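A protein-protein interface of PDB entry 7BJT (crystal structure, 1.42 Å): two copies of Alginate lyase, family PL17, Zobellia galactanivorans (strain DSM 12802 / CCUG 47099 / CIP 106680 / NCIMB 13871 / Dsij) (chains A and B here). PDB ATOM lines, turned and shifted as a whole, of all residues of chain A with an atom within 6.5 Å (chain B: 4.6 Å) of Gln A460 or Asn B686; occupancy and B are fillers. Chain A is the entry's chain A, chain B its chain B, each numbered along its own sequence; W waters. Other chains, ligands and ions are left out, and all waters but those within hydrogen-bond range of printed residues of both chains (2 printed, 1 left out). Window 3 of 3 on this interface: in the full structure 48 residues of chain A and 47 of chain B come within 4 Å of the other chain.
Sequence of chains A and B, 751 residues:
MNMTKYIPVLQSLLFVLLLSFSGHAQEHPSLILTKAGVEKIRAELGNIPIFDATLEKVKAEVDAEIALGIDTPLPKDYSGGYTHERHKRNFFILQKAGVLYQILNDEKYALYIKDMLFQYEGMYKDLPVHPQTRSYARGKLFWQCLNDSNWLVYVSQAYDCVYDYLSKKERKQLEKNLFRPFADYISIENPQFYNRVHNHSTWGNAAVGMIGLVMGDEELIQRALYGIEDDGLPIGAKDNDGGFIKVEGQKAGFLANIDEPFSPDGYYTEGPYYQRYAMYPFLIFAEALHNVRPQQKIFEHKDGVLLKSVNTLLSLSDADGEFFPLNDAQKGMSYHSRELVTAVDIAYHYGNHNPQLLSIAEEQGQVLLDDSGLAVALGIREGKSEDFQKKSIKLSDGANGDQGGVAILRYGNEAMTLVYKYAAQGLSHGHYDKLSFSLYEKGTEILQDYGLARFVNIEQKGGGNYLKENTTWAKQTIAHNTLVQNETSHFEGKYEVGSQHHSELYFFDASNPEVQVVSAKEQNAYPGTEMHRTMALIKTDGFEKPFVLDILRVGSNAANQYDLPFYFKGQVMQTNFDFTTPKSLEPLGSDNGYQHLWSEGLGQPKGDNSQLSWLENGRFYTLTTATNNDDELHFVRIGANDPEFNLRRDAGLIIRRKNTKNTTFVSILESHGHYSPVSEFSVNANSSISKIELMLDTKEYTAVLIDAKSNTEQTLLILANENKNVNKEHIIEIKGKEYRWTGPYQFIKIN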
ATOM      1  N   SER A  79     -20.830   0.662  16.718  1.00  0.00           N
ATOM      2  CA  SER A  79     -19.506   0.190  16.328  1.00  0.00           C
ATOM      3  C   SER A  79     -18.535   0.100  17.500  1.00  0.00           C
ATOM      4  O   SER A  79     -18.559   0.925  18.419  1.00  0.00           O
ATOM      5  CB  SER A  79     -18.927   1.037  15.194  1.00  0.00           C
ATOM      6  OG  SER A  79     -18.592   2.354  15.603  1.00  0.00           O
ATOM      7  N   GLY A  80     -17.717  -0.948  17.483  1.00  0.00           N
ATOM      8  CA  GLY A  80     -16.846  -1.281  18.612  1.00  0.00           C
ATOM      9  C   GLY A  80     -17.511  -2.119  19.689  1.00  0.00           C
ATOM     10  O   GLY A  80     -16.823  -2.777  20.473  1.00  0.00           O
ATOM     11  N   ASN A 457     -15.069   3.581  14.692  1.00  0.00           N
ATOM     12  CA  ASN A 457     -15.362   2.269  15.276  1.00  0.00           C
ATOM     13  C   ASN A 457     -14.845   2.076  16.703  1.00  0.00           C
ATOM     14  O   ASN A 457     -14.770   0.939  17.172  1.00  0.00           O
ATOM     15  CB  ASN A 457     -14.886   1.095  14.385  1.00  0.00           C
ATOM     16  CG  ASN A 457     -15.451   1.135  12.982  1.00  0.00           C
ATOM     17  OD1 ASN A 457     -16.607   1.517  12.767  1.00  0.00           O
ATOM     18  ND2 ASN A 457     -14.655   0.683  12.015  1.00  0.00           N
ATOM     19  N   ILE A 458     -14.521   3.165  17.401  1.00  0.00           N
ATOM     20  CA  ILE A 458     -14.178   3.083  18.826  1.00  0.00           C
ATOM     21  C   ILE A 458     -15.423   3.452  19.622  1.00  0.00           C
ATOM     22  O   ILE A 458     -15.845   4.612  19.653  1.00  0.00           O
ATOM     23  CB  ILE A 458     -12.967   3.966  19.205  1.00  0.00           C
ATOM     24  CG1 ILE A 458     -11.748   3.557  18.362  1.00  0.00           C
ATOM     25  CG2 ILE A 458     -12.692   3.852  20.705  1.00  0.00           C
ATOM     26  CD1 ILE A 458     -10.436   4.246  18.697  1.00  0.00           C
ATOM     27  N   GLU A 459     -16.000   2.446  20.283  1.00  0.00           N
ATOM     28  CA  GLU A 459     -17.307   2.583  20.933  1.00  0.00           C
ATOM     29  C   GLU A 459     -17.331   3.680  21.997  1.00  0.00           C
ATOM     30  O   GLU A 459     -18.336   4.372  22.171  1.00  0.00           O
ATOM     31  CB  GLU A 459     -17.710   1.257  21.583  1.00  0.00           C
ATOM     32  CG  GLU A 459     -19.182   1.155  21.946  1.00  0.00           C
ATOM     33  CD  GLU A 459     -19.516  -0.078  22.759  1.00  0.00           C
ATOM     34  OE1 GLU A 459     -18.600  -0.766  23.280  1.00  0.00           O
ATOM     35  OE2 GLU A 459     -20.715  -0.383  22.845  1.00  0.00           O
ATOM     36  N   GLN A 460     -16.199   3.840  22.677  1.00  0.00           N
ATOM     37  CA  GLN A 460     -16.052   4.770  23.791  1.00  0.00           C
ATOM     38  C   GLN A 460     -16.165   6.233  23.359  1.00  0.00           C
ATOM     39  O   GLN A 460     -16.436   7.108  24.185  1.00  0.00           O
ATOM     40  CB  GLN A 460     -14.689   4.562  24.469  1.00  0.00           C
ATOM     41  CG  GLN A 460     -14.545   3.282  25.288  1.00  0.00           C
ATOM     42  CD  GLN A 460     -14.582   2.002  24.455  1.00  0.00           C
ATOM     43  OE1 GLN A 460     -14.165   1.979  23.296  1.00  0.00           O
ATOM     44  NE2 GLN A 460     -15.100   0.932  25.041  1.00  0.00           N
ATOM     45  N   LYS A 461     -15.934   6.498  22.075  1.00  0.00           N
ATOM     46  CA  LYS A 461     -16.076   7.832  21.508  1.00  0.00           C
ATOM     47  C   LYS A 461     -17.361   7.929  20.709  1.00  0.00           C
ATOM     48  O   LYS A 461     -17.377   7.735  19.500  1.00  0.00           O
ATOM     49  CB  LYS A 461     -14.861   8.142  20.629  1.00  0.00           C
ATOM     50  CG  LYS A 461     -13.619   8.446  21.432  1.00  0.00           C
ATOM     51  CD  LYS A 461     -13.804   9.813  22.081  1.00  0.00           C
ATOM     52  CE  LYS A 461     -12.539  10.414  22.588  1.00  0.00           C
ATOM     53  NZ  LYS A 461     -12.837  11.405  23.646  1.00  0.00           N
ATOM     54  N   GLY A 462     -18.456   8.213  21.399  1.00  0.00           N
ATOM     55  CA  GLY A 462     -19.737   8.407  20.733  1.00  0.00           C
ATOM     56  C   GLY A 462     -20.156   7.257  19.831  1.00  0.00           C
ATOM     57  O   GLY A 462     -20.664   7.476  18.740  1.00  0.00           O
ATOM     58  N   GLY A 463     -19.933   6.028  20.283  1.00  0.00           N
ATOM     59  CA  GLY A 463     -20.286   4.839  19.510  1.00  0.00           C
ATOM     60  C   GLY A 463     -19.490   4.646  18.237  1.00  0.00           C
ATOM     61  O   GLY A 463     -19.925   3.926  17.336  1.00  0.00           O
ATOM     62  N   GLY A 464     -18.320   5.286  18.166  1.00  0.00           N
ATOM     63  CA  GLY A 464     -17.471   5.258  16.985  1.00  0.00           C
ATOM     64  C   GLY A 464     -17.986   6.062  15.814  1.00  0.00           C
ATOM     65  O   GLY A 464     -17.464   5.929  14.715  1.00  0.00           O
ATOM     66  N   MET B 573      -9.975   8.424  26.209  1.00  0.00           N
ATOM     67  CA  MET B 573     -11.047   7.585  25.659  1.00  0.00           C
ATOM     68  C   MET B 573     -12.313   7.557  26.497  1.00  0.00           C
ATOM     69  O   MET B 573     -13.410   7.643  25.942  1.00  0.00           O
ATOM     70  CB  MET B 573     -10.537   6.156  25.465  1.00  0.00           C
ATOM     71  CG  MET B 573      -9.581   6.038  24.290  1.00  0.00           C
ATOM     72  SD  MET B 573     -10.466   6.081  22.725  1.00  0.00           S
ATOM     73  CE  MET B 573      -9.651   7.411  21.871  1.00  0.00           C
ATOM     74  N   GLN B 574     -12.188   7.391  27.810  1.00  0.00           N
ATOM     75  CA  GLN B 574     -13.372   7.267  28.669  1.00  0.00           C
ATOM     76  C   GLN B 574     -13.003   7.526  30.122  1.00  0.00           C
ATOM     77  O   GLN B 574     -11.857   7.315  30.529  1.00  0.00           O
ATOM     78  CB  GLN B 574     -14.016   5.864  28.498  1.00  0.00           C
ATOM     79  CG  GLN B 574     -15.308   5.583  29.291  1.00  0.00           C
ATOM     80  CD  GLN B 574     -16.615   5.884  28.553  1.00  0.00           C
ATOM     81  OE1 GLN B 574     -16.738   5.626  27.349  1.00  0.00           O
ATOM     82  NE2 GLN B 574     -17.616   6.408  29.282  1.00  0.00           N
ATOM     83  N   HIS B 672      -4.370  -2.916  27.631  1.00  0.00           N
ATOM     84  CA  HIS B 672      -5.309  -3.875  27.053  1.00  0.00           C
ATOM     85  C   HIS B 672      -5.694  -3.494  25.648  1.00  0.00           C
ATOM     86  O   HIS B 672      -5.816  -2.314  25.317  1.00  0.00           O
ATOM     87  CB  HIS B 672      -6.563  -4.019  27.935  1.00  0.00           C
ATOM     88  CG  HIS B 672      -7.199  -2.716  28.305  1.00  0.00           C
ATOM     89  ND1 HIS B 672      -8.173  -2.113  27.533  1.00  0.00           N
ATOM     90  CD2 HIS B 672      -7.003  -1.900  29.366  1.00  0.00           C
ATOM     91  CE1 HIS B 672      -8.545  -0.983  28.110  1.00  0.00           C
ATOM     92  NE2 HIS B 672      -7.846  -0.829  29.218  1.00  0.00           N
ATOM     93  N   ASN B 684     -10.788  -5.157  22.692  1.00  0.00           N
ATOM     94  CA  ASN B 684     -10.560  -5.132  24.137  1.00  0.00           C
ATOM     95  C   ASN B 684     -10.247  -3.741  24.677  1.00  0.00           C
ATOM     96  O   ASN B 684      -9.224  -3.504  25.339  1.00  0.00           O
ATOM     97  CB  ASN B 684      -9.479  -6.147  24.522  1.00  0.00           C
ATOM     98  CG  ASN B 684      -9.887  -7.586  24.234  1.00  0.00           C
ATOM     99  OD1 ASN B 684      -9.055  -8.393  23.820  1.00  0.00           O
ATOM    100  ND2 ASN B 684     -11.149  -7.917  24.464  1.00  0.00           N
ATOM    101  N   ALA B 685     -11.168  -2.825  24.397  1.00  0.00           N
ATOM    102  CA  ALA B 685     -11.017  -1.418  24.733  1.00  0.00           C
ATOM    103  C   ALA B 685     -11.429  -1.067  26.159  1.00  0.00           C
ATOM    104  O   ALA B 685     -11.197   0.051  26.597  1.00  0.00           O
ATOM    105  CB  ALA B 685     -11.803  -0.569  23.738  1.00  0.00           C
ATOM    106  N   ASN B 686     -12.038  -1.999  26.884  1.00  0.00           N
ATOM    107  CA  ASN B 686     -12.439  -1.752  28.266  1.00  0.00           C
ATOM    108  C   ASN B 686     -11.505  -2.418  29.255  1.00  0.00           C
ATOM    109  O   ASN B 686     -10.858  -3.411  28.946  1.00  0.00           O
ATOM    110  CB  ASN B 686     -13.860  -2.262  28.519  1.00  0.00           C
ATOM    111  CG  ASN B 686     -14.904  -1.522  27.712  1.00  0.00           C
ATOM    112  OD1 ASN B 686     -15.651  -2.139  26.961  1.00  0.00           O
ATOM    113  ND2 ASN B 686     -14.981  -0.213  27.881  1.00  0.00           N
ATOM    114  N   SER B 687     -11.471  -1.855  30.456  1.00  0.00           N
ATOM    115  CA  SER B 687     -10.741  -2.415  31.587  1.00  0.00           C
ATOM    116  C   SER B 687     -11.273  -3.799  31.960  1.00  0.00           C
ATOM    117  O   SER B 687     -12.446  -4.098  31.741  1.00  0.00           O
ATOM    118  CB  SER B 687     -10.906  -1.474  32.778  1.00  0.00           C
ATOM    119  OG  SER B 687     -10.367  -2.008  33.969  1.00  0.00           O
ATOM    120  N   SER B 688     -10.398  -4.634  32.511  1.00  0.00           N
ATOM    121  CA  SER B 688     -10.813  -5.903  33.129  1.00  0.00           C
ATOM    122  C   SER B 688     -10.916  -5.824  34.658  1.00  0.00           C
ATOM    123  O   SER B 688     -11.196  -6.836  35.304  1.00  0.00           O
ATOM    124  CB  SER B 688      -9.861  -7.029  32.713  1.00  0.00           C
ATOM    125  OG  SER B 688     -10.048  -7.366  31.343  1.00  0.00           O
ATOM    126  N   LYS B 709     -13.075  -8.672  36.086  1.00  0.00           N
ATOM    127  CA  LYS B 709     -14.453  -8.719  35.590  1.00  0.00           C
ATOM    128  C   LYS B 709     -14.831 -10.098  35.041  1.00  0.00           C
ATOM    129  O   LYS B 709     -16.027 -10.438  35.016  1.00  0.00           O
ATOM    130  CB  LYS B 709     -14.732  -7.581  34.575  1.00  0.00           C
ATOM    131  CG  LYS B 709     -15.183  -6.281  35.249  1.00  0.00           C
ATOM    132  CD  LYS B 709     -15.742  -5.237  34.279  1.00  0.00           C
ATOM    133  CE  LYS B 709     -14.780  -4.084  34.044  1.00  0.00           C
ATOM    134  NZ  LYS B 709     -15.031  -3.312  32.792  1.00  0.00           N
HETATM  135  O   HOH W   1     -14.472  10.225  25.475  1.00  0.00           O
HETATM  136  O   HOH W   2     -11.663   3.204  23.881  1.00  0.00           O
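Gly A80 touches none of the printed residues of chain B.
Gln A460 touches just these residues of chain B: Met B573 (3.5 Å), Gln B574 (3.5 Å), Ala B685 (3.5 Å) and Asn B686 (3.1 Å).
Of the printed residues of chain A, Met B573 touches Ile A458 and Gln A460.
Printed residues of chain A within 4 Å of Ala B685: Gln A460 (3.5 Å).
Lys B709 touches none of the printed residues of chain A.
The nearest residue of chain A that does not touch Asn B686 is Glu A459 (4.9 Å).
The nearest printed residue of chain B that does not touch Ile A458 is Ala B685 (5.4 Å).
Water W1 bridges NZ of Lys A461 (2.7 Å) and O of Met B573 (2.8 Å).
Water W2 bridges OE1 of Gln A460 (2.8 Å) and SD of Met B573 (3.3 Å).
NE2 of Gln A460 sits close to ND2 of Asn B686.
Printed residues of chain B that touch a printed residue of chain A: Met B573, Gln B574, Ala B685 and Asn B686.
Hydrophobic or aromatic side chains of chain B within 4 Å of the printed part of chain A: Met B573 and Ala B685.
Among the printed residues, no Asp or Glu carboxylate lies within 4 Å of a Lys or Arg side-chain nitrogen of the other chain.
Among the printed residues, pairs that only touch across the chains: Gln A460 with Ala B685 (3.5 Å), Gln A460 with Gln B574 (3.5 Å), Gln A460 with Met B573 (3.5 Å) and Ile A458 with Met B573 (3.7 Å).
No position is printed for both chains.
O of Ile A458 is in hydrogen-bond range of N of Gly A464, at 3.0 Å.
ND1 of His B672 lies within hydrogen-bond range of O of Asn B686 (3.3 Å).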
